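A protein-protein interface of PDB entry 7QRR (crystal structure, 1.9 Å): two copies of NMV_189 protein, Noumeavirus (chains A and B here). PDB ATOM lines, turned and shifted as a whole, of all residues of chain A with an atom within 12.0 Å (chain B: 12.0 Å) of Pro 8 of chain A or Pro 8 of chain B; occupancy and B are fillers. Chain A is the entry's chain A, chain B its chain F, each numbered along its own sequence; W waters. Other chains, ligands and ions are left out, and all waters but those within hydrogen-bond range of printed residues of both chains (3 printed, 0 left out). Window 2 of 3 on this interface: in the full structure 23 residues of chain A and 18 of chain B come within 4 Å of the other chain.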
ATOM      1  N   VAL A   7       7.244  22.333  -9.220  1.00  0.00           N
ATOM      2  CA  VAL A   7       8.386  22.556  -8.341  1.00  0.00           C
ATOM      3  C   VAL A   7       9.466  23.364  -9.061  1.00  0.00           C
ATOM      4  O   VAL A   7       9.874  23.024 -10.171  1.00  0.00           O
ATOM      5  CB  VAL A   7       8.993  21.228  -7.837  1.00  0.00           C
ATOM      6  CG1 VAL A   7      10.213  21.493  -6.955  1.00  0.00           C
ATOM      7  CG2 VAL A   7       7.952  20.414  -7.084  1.00  0.00           C
ATOM      8  N   PRO A   8       9.935  24.445  -8.426  1.00  0.00           N
ATOM      9  CA  PRO A   8      10.926  25.316  -9.059  1.00  0.00           C
ATOM     10  C   PRO A   8      12.295  24.671  -9.174  1.00  0.00           C
ATOM     11  O   PRO A   8      12.656  23.794  -8.387  1.00  0.00           O
ATOM     12  CB  PRO A   8      10.982  26.520  -8.116  1.00  0.00           C
ATOM     13  CG  PRO A   8      10.598  25.962  -6.790  1.00  0.00           C
ATOM     14  CD  PRO A   8       9.539  24.939  -7.097  1.00  0.00           C
ATOM     15  N   THR A   9      13.046  25.119 -10.171  1.00  0.00           N
ATOM     16  CA  THR A   9      14.450  24.783 -10.304  1.00  0.00           C
ATOM     17  C   THR A   9      15.268  26.065 -10.174  1.00  0.00           C
ATOM     18  O   THR A   9      14.732  27.168 -10.340  1.00  0.00           O
ATOM     19  CB  THR A   9      14.750  24.112 -11.652  1.00  0.00           C
ATOM     20  OG1 THR A   9      14.484  25.039 -12.712  1.00  0.00           O
ATOM     21  CG2 THR A   9      13.874  22.886 -11.844  1.00  0.00           C
ATOM     22  N   VAL A  10      16.552  25.924  -9.870  1.00  0.00           N
ATOM     23  CA  VAL A  10      17.451  27.071  -9.823  1.00  0.00           C
ATOM     24  C   VAL A  10      18.612  26.855 -10.789  1.00  0.00           C
ATOM     25  O   VAL A  10      19.223  25.782 -10.825  1.00  0.00           O
ATOM     26  CB  VAL A  10      17.981  27.336  -8.388  1.00  0.00           C
ATOM     27  CG1 VAL A  10      18.726  26.125  -7.833  1.00  0.00           C
ATOM     28  CG2 VAL A  10      18.870  28.584  -8.362  1.00  0.00           C
ATOM     29  N   THR A  11      18.882  27.871 -11.602  1.00  0.00           N
ATOM     30  CA  THR A  11      19.973  27.842 -12.555  1.00  0.00           C
ATOM     31  C   THR A  11      20.784  29.107 -12.353  1.00  0.00           C
ATOM     32  O   THR A  11      20.224  30.200 -12.407  1.00  0.00           O
ATOM     33  CB  THR A  11      19.472  27.786 -14.007  1.00  0.00           C
ATOM     34  OG1 THR A  11      18.478  26.761 -14.140  1.00  0.00           O
ATOM     35  CG2 THR A  11      20.624  27.513 -14.960  1.00  0.00           C
ATOM     36  N   THR A  12      22.081  28.962 -12.108  1.00  0.00           N
ATOM     37  CA  THR A  12      22.968  30.120 -11.960  1.00  0.00           C
ATOM     38  C   THR A  12      24.166  29.952 -12.888  1.00  0.00           C
ATOM     39  O   THR A  12      24.892  28.954 -12.807  1.00  0.00           O
ATOM     40  CB  THR A  12      23.436  30.296 -10.498  1.00  0.00           C
ATOM     41  OG1 THR A  12      22.301  30.502  -9.644  1.00  0.00           O
ATOM     42  CG2 THR A  12      24.385  31.477 -10.367  1.00  0.00           C
ATOM     43  N   THR A  45      20.970  34.437 -12.582  1.00  0.00           N
ATOM     44  CA  THR A  45      20.365  33.315 -11.894  1.00  0.00           C
ATOM     45  C   THR A  45      18.862  33.362 -12.136  1.00  0.00           C
ATOM     46  O   THR A  45      18.256  34.435 -12.224  1.00  0.00           O
ATOM     47  CB  THR A  45      20.693  33.335 -10.374  1.00  0.00           C
ATOM     48  OG1 THR A  45      20.146  32.177  -9.739  1.00  0.00           O
ATOM     49  CG2 THR A  45      20.139  34.587  -9.704  1.00  0.00           C
ATOM     50  N   ARG A  46      18.271  32.189 -12.308  1.00  0.00           N
ATOM     51  CA  ARG A  46      16.833  32.065 -12.422  1.00  0.00           C
ATOM     52  C   ARG A  46      16.331  31.022 -11.436  1.00  0.00           C
ATOM     53  O   ARG A  46      16.810  29.888 -11.442  1.00  0.00           O
ATOM     54  CB  ARG A  46      16.430  31.681 -13.845  1.00  0.00           C
ATOM     55  CG  ARG A  46      14.939  31.409 -13.981  1.00  0.00           C
ATOM     56  CD  ARG A  46      14.519  31.135 -15.421  1.00  0.00           C
ATOM     57  NE  ARG A  46      13.068  30.994 -15.511  1.00  0.00           N
ATOM     58  CZ  ARG A  46      12.382  30.938 -16.651  1.00  0.00           C
ATOM     59  NH1 ARG A  46      13.008  31.025 -17.813  1.00  0.00           N
ATOM     60  NH2 ARG A  46      11.065  30.814 -16.623  1.00  0.00           N
ATOM     61  N   VAL A  47      15.400  31.410 -10.572  1.00  0.00           N
ATOM     62  CA  VAL A  47      14.732  30.445  -9.699  1.00  0.00           C
ATOM     63  C   VAL A  47      13.234  30.580  -9.946  1.00  0.00           C
ATOM     64  O   VAL A  47      12.678  31.673  -9.856  1.00  0.00           O
ATOM     65  CB  VAL A  47      15.101  30.646  -8.199  1.00  0.00           C
ATOM     66  CG1 VAL A  47      14.812  32.078  -7.721  1.00  0.00           C
ATOM     67  CG2 VAL A  47      14.393  29.621  -7.319  1.00  0.00           C
ATOM     68  N   GLY A  48      12.586  29.477 -10.329  1.00  0.00           N
ATOM     69  CA  GLY A  48      11.210  29.557 -10.790  1.00  0.00           C
ATOM     70  C   GLY A  48      11.159  30.430 -12.031  1.00  0.00           C
ATOM     71  O   GLY A  48      11.871  30.174 -12.997  1.00  0.00           O
ATOM     72  N   ASP A  49      10.336  31.478 -12.001  1.00  0.00           N
ATOM     73  CA  ASP A  49      10.251  32.400 -13.130  1.00  0.00           C
ATOM     74  C   ASP A  49      10.915  33.736 -12.806  1.00  0.00           C
ATOM     75  O   ASP A  49      10.667  34.734 -13.481  1.00  0.00           O
ATOM     76  CB  ASP A  49       8.791  32.633 -13.531  1.00  0.00           C
ATOM     77  CG  ASP A  49       8.169  31.412 -14.194  1.00  0.00           C
ATOM     78  OD1 ASP A  49       8.922  30.609 -14.779  1.00  0.00           O
ATOM     79  OD2 ASP A  49       6.934  31.253 -14.115  1.00  0.00           O
ATOM     80  N   THR A  50      11.753  33.746 -11.775  1.00  0.00           N
ATOM     81  CA  THR A  50      12.354  34.985 -11.305  1.00  0.00           C
ATOM     82  C   THR A  50      13.821  35.030 -11.688  1.00  0.00           C
ATOM     83  O   THR A  50      14.611  34.168 -11.287  1.00  0.00           O
ATOM     84  CB  THR A  50      12.181  35.134  -9.794  1.00  0.00           C
ATOM     85  OG1 THR A  50      10.782  35.059  -9.492  1.00  0.00           O
ATOM     86  CG2 THR A  50      12.733  36.475  -9.310  1.00  0.00           C
ATOM     87  N   ALA A  51      14.170  36.030 -12.495  1.00  0.00           N
ATOM     88  CA  ALA A  51      15.520  36.168 -13.038  1.00  0.00           C
ATOM     89  C   ALA A  51      16.240  37.349 -12.404  1.00  0.00           C
ATOM     90  O   ALA A  51      15.669  38.436 -12.294  1.00  0.00           O
ATOM     91  CB  ALA A  51      15.464  36.336 -14.557  1.00  0.00           C
ATOM     92  N   PRO B   6      20.784  21.111  -7.945  1.00  0.00           N
ATOM     93  CA  PRO B   6      19.853  20.596  -6.934  1.00  0.00           C
ATOM     94  C   PRO B   6      18.570  21.423  -6.828  1.00  0.00           C
ATOM     95  O   PRO B   6      18.449  22.478  -7.457  1.00  0.00           O
ATOM     96  CB  PRO B   6      20.660  20.686  -5.632  1.00  0.00           C
ATOM     97  CG  PRO B   6      22.086  20.663  -6.064  1.00  0.00           C
ATOM     98  CD  PRO B   6      22.123  21.372  -7.387  1.00  0.00           C
ATOM     99  N   VAL B   7      17.627  20.929  -6.029  1.00  0.00           N
ATOM    100  CA  VAL B   7      16.359  21.605  -5.776  1.00  0.00           C
ATOM    101  C   VAL B   7      16.563  22.800  -4.845  1.00  0.00           C
ATOM    102  O   VAL B   7      17.277  22.696  -3.846  1.00  0.00           O
ATOM    103  CB  VAL B   7      15.319  20.621  -5.165  1.00  0.00           C
ATOM    104  CG1 VAL B   7      14.153  21.361  -4.509  1.00  0.00           C
ATOM    105  CG2 VAL B   7      14.814  19.654  -6.231  1.00  0.00           C
ATOM    106  N   PRO B   8      15.947  23.943  -5.185  1.00  0.00           N
ATOM    107  CA  PRO B   8      15.996  25.149  -4.353  1.00  0.00           C
ATOM    108  C   PRO B   8      15.485  24.934  -2.938  1.00  0.00           C
ATOM    109  O   PRO B   8      14.596  24.115  -2.709  1.00  0.00           O
ATOM    110  CB  PRO B   8      15.078  26.135  -5.092  1.00  0.00           C
ATOM    111  CG  PRO B   8      14.347  25.331  -6.125  1.00  0.00           C
ATOM    112  CD  PRO B   8      15.244  24.179  -6.455  1.00  0.00           C
ATOM    113  N   THR B   9      16.057  25.680  -2.002  1.00  0.00           N
ATOM    114  CA  THR B   9      15.514  25.795  -0.656  1.00  0.00           C
ATOM    115  C   THR B   9      15.061  27.244  -0.432  1.00  0.00           C
ATOM    116  O   THR B   9      15.536  28.153  -1.120  1.00  0.00           O
ATOM    117  CB  THR B   9      16.551  25.394   0.407  1.00  0.00           C
ATOM    118  OG1 THR B   9      17.679  26.272   0.320  1.00  0.00           O
ATOM    119  CG2 THR B   9      17.022  23.957   0.184  1.00  0.00           C
ATOM    120  N   VAL B  10      14.131  27.447   0.496  1.00  0.00           N
ATOM    121  CA  VAL B  10      13.725  28.791   0.916  1.00  0.00           C
ATOM    122  C   VAL B  10      14.046  29.002   2.379  1.00  0.00           C
ATOM    123  O   VAL B  10      13.743  28.154   3.212  1.00  0.00           O
ATOM    124  CB  VAL B  10      12.227  29.038   0.717  1.00  0.00           C
ATOM    125  CG1 VAL B  10      11.870  30.486   1.059  1.00  0.00           C
ATOM    126  CG2 VAL B  10      11.865  28.761  -0.677  1.00  0.00           C
ATOM    127  N   THR B  11      14.663  30.137   2.685  1.00  0.00           N
ATOM    128  CA  THR B  11      15.001  30.496   4.053  1.00  0.00           C
ATOM    129  C   THR B  11      14.590  31.941   4.288  1.00  0.00           C
ATOM    130  O   THR B  11      15.021  32.825   3.551  1.00  0.00           O
ATOM    131  CB  THR B  11      16.508  30.342   4.331  1.00  0.00           C
ATOM    132  OG1 THR B  11      16.943  29.025   3.952  1.00  0.00           O
ATOM    133  CG2 THR B  11      16.810  30.586   5.808  1.00  0.00           C
ATOM    134  N   THR B  12      13.758  32.178   5.299  1.00  0.00           N
ATOM    135  CA  THR B  12      13.304  33.525   5.621  1.00  0.00           C
ATOM    136  C   THR B  12      13.558  33.777   7.098  1.00  0.00           C
ATOM    137  O   THR B  12      13.108  33.008   7.944  1.00  0.00           O
ATOM    138  CB  THR B  12      11.811  33.716   5.277  1.00  0.00           C
ATOM    139  OG1 THR B  12      11.610  33.462   3.882  1.00  0.00           O
ATOM    140  CG2 THR B  12      11.344  35.135   5.604  1.00  0.00           C
ATOM    141  N   THR B  45      15.200  37.091   2.974  1.00  0.00           N
ATOM    142  CA  THR B  45      14.793  35.783   2.505  1.00  0.00           C
ATOM    143  C   THR B  45      15.701  35.395   1.353  1.00  0.00           C
ATOM    144  O   THR B  45      16.161  36.247   0.594  1.00  0.00           O
ATOM    145  CB  THR B  45      13.315  35.741   2.066  1.00  0.00           C
ATOM    146  OG1 THR B  45      12.974  34.405   1.678  1.00  0.00           O
ATOM    147  CG2 THR B  45      13.058  36.677   0.886  1.00  0.00           C
ATOM    148  N   ARG B  46      15.992  34.107   1.247  1.00  0.00           N
ATOM    149  CA  ARG B  46      16.768  33.595   0.129  1.00  0.00           C
ATOM    150  C   ARG B  46      16.073  32.374  -0.440  1.00  0.00           C
ATOM    151  O   ARG B  46      15.786  31.422   0.286  1.00  0.00           O
ATOM    152  CB  ARG B  46      18.195  33.241   0.561  1.00  0.00           C
ATOM    153  CG  ARG B  46      19.023  32.614  -0.542  1.00  0.00           C
ATOM    154  CD  ARG B  46      20.446  32.314  -0.095  1.00  0.00           C
ATOM    155  NE  ARG B  46      21.226  31.725  -1.181  1.00  0.00           N
ATOM    156  CZ  ARG B  46      22.546  31.574  -1.151  1.00  0.00           C
ATOM    157  NH1 ARG B  46      23.225  31.975  -0.089  1.00  0.00           N
ATOM    158  NH2 ARG B  46      23.188  31.037  -2.181  1.00  0.00           N
ATOM    159  N   VAL B  47      15.784  32.412  -1.731  1.00  0.00           N
ATOM    160  CA  VAL B  47      15.291  31.238  -2.430  1.00  0.00           C
ATOM    161  C   VAL B  47      16.239  30.972  -3.601  1.00  0.00           C
ATOM    162  O   VAL B  47      16.527  31.872  -4.397  1.00  0.00           O
ATOM    163  CB  VAL B  47      13.824  31.423  -2.894  1.00  0.00           C
ATOM    164  CG1 VAL B  47      13.667  32.667  -3.792  1.00  0.00           C
ATOM    165  CG2 VAL B  47      13.319  30.166  -3.605  1.00  0.00           C
ATOM    166  N   GLY B  48      16.760  29.748  -3.685  1.00  0.00           N
ATOM    167  CA  GLY B  48      17.851  29.456  -4.599  1.00  0.00           C
ATOM    168  C   GLY B  48      19.044  30.353  -4.286  1.00  0.00           C
ATOM    169  O   GLY B  48      19.514  30.393  -3.149  1.00  0.00           O
ATOM    170  N   ASP B  49      19.518  31.093  -5.286  1.00  0.00           N
ATOM    171  CA  ASP B  49      20.609  32.048  -5.085  1.00  0.00           C
ATOM    172  C   ASP B  49      20.107  33.490  -5.044  1.00  0.00           C
ATOM    173  O   ASP B  49      20.889  34.421  -5.195  1.00  0.00           O
ATOM    174  CB  ASP B  49      21.656  31.900  -6.198  1.00  0.00           C
ATOM    175  CG  ASP B  49      22.429  30.599  -6.088  1.00  0.00           C
ATOM    176  OD1 ASP B  49      22.522  30.101  -4.954  1.00  0.00           O
ATOM    177  OD2 ASP B  49      22.935  30.086  -7.116  1.00  0.00           O
ATOM    178  N   THR B  50      18.809  33.667  -4.822  1.00  0.00           N
ATOM    179  CA  THR B  50      18.200  34.991  -4.881  1.00  0.00           C
ATOM    180  C   THR B  50      17.802  35.506  -3.497  1.00  0.00           C
ATOM    181  O   THR B  50      16.913  34.957  -2.845  1.00  0.00           O
ATOM    182  CB  THR B  50      16.993  34.964  -5.803  1.00  0.00           C
ATOM    183  OG1 THR B  50      17.417  34.457  -7.075  1.00  0.00           O
ATOM    184  CG2 THR B  50      16.407  36.375  -5.988  1.00  0.00           C
ATOM    185  N   ALA B  51      18.473  36.576  -3.072  1.00  0.00           N
ATOM    186  CA  ALA B  51      18.300  37.170  -1.750  1.00  0.00           C
ATOM    187  C   ALA B  51      17.488  38.463  -1.823  1.00  0.00           C
ATOM    188  O   ALA B  51      17.730  39.299  -2.688  1.00  0.00           O
ATOM    189  CB  ALA B  51      19.661  37.456  -1.118  1.00  0.00           C
HETATM  190  O   HOH W   1      18.222  31.902  -7.728  1.00  0.00           O
HETATM  191  O   HOH W   2      16.936  22.999  -9.355  1.00  0.00           O
HETATM  192  O   HOH W   3      16.277  35.569  -9.323  1.00  0.00           O
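Among the printed residues, pairs that only touch across the chains: Pro 8 of chain A with Pro 8 of chain B (3.2 Å), Val 47 of chain A with Thr 50 of chain B (3.6 Å), Val 10 of chain A with Pro 6 of chain B (3.7 Å), Val 47 of chain A with Val 47 of chain B (3.7 Å), Thr 45 of chain A with Thr 50 of chain B (3.8 Å), Thr 45 of chain A with Asp 49 of chain B (3.9 Å), Thr 9 of chain A with Pro 8 of chain B (3.98 Å) and Val 10 of chain A with Gly 48 of chain B (3.99 Å).
The guanidinium group of Arg 46 of chain B is in hydrogen-bond range of the backbone carbonyl oxygen of Gly 48 of chain B (2.9 Å).
The guanidinium group (NH2) of Arg 46 of chain B lies within salt-bridge range of the side-chain carboxylate (OD1) of Asp 49 of chain B.
The side-chain hydroxyl (OG1) of Thr 12 of chain A is in hydrogen-bond range of the side-chain hydroxyl (OG1) of Thr 45 of chain A, at 2.7 Å.
The backbone NH (N) of Gly 48 of chain B lies within hydrogen-bond range of the backbone carbonyl oxygen (O) of Thr 9 of chain B, 3.3 Å away.
O of Thr 11 of chain A lies close to OG1 of Thr 45 of chain A, at 3.3 Å.
The backbone carbonyl oxygen (O) of Thr 9 of chain A sits at hydrogen-bond distance from the backbone NH (N) of Gly 48 of chain A (3.2 Å).
Pro 8 of chain A touches its own counterpart, Pro 8 of chain B.
Val 10 of chain A touches Gly 48 of chain B, but with the chains exchanged Gly 48 of chain A does not touch Val 10 of chain B (9.7 Å).
Thr 45 of chain A touches Thr 50 of chain B, but with the chains exchanged Thr 50 of chain A does not touch Thr 45 of chain B (10.2 Å).
Val 47 of chain A touches Thr 50 of chain B, but with the chains exchanged Thr 50 of chain A does not touch Val 47 of chain B (6.7 Å).
Positions printed for both chains: 7, 8, 9, 10, 11, 12, 45, 46, 47, 48, 49, 50 and 51.
Of the 9 pairs that touch across the chains among the printed residues, 2 have their exchanged pair printed and touching as well.
The side-chain carboxylate (OD2) of Asp 49 of chain B is in hydrogen-bond range of the side-chain hydroxyl (OG1) of Thr 12 of chain A, 2.6 Å away.
No residue of chain B comes within 4 Å of Val 7 of chain A.
Pro 8 of chain A touches one residue of chain B.
Thr 9 of chain A touches just one residue of chain B: Pro 8.
Printed residues of chain B within 4 Å of Thr 12 of chain A: Asp 49.
Of the printed residues of chain B, Thr 45 of chain A touches Asp 49 and Thr 50.
Of chain B, only Val 47 and Thr 50 come within 4 Å of Val 47 of chain A.
Gly 48 of chain A touches none of the printed residues of chain B.
Printed residues of chain A within 4 Å of Pro 6 of chain B: Val 10.
No residue of chain A comes within 4 Å of Val 7 of chain B.
Of the printed residues of chain A, Pro 8 of chain B touches Pro 8 (3.2 Å) and Thr 9 (3.98 Å).
Thr 9 of chain B touches none of the printed residues of chain A.
Thr 12 of chain B touches none of the printed residues of chain A.
Val 47 of chain B touches just one residue of chain A: Val 47.
Printed residues of chain A within 4 Å of Gly 48 of chain B: Val 10 (3.99 Å).
Printed residues of chain A within 4 Å of Asp 49 of chain B: Thr 12 (2.6 Å) and Thr 45 (3.9 Å).
The nearest printed residue of chain A that does not touch Pro 8 of chain B is Val 10 of chain A (4.1 Å).
Water W2 lies within hydrogen-bond range of the backbone carbonyl oxygen of Pro 6 of chain B and the backbone NH of Val 10 of chain A.
Water W3 bridges OG1 of Thr 50 of chain B and O of Thr 50 of chain A.
Water W1 lies within hydrogen-bond range of OG1 of Thr 50 of chain B, OG1 of Thr 45 of chain A and N of Asp 49 of chain B.
Of the 13 printed residues of chain A, 6 touch a printed residue of chain B.
Printed residues of chain A that touch a printed residue of chain B: Pro 8, Thr 9, Val 10, Thr 12, Thr 45 and Val 47.
Hydrophobic or aromatic side chains of chain A within 4 Å of the printed part of chain B: Pro 8, Val 10 and Val 47.
Hydrophobic or aromatic side chains of chain B within 4 Å of the printed part of chain A: Pro 8 and Val 47.
Among the printed residues, no Asp or Glu carboxylate lies within 4 Å of a Lys or Arg side-chain nitrogen of the other chain.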
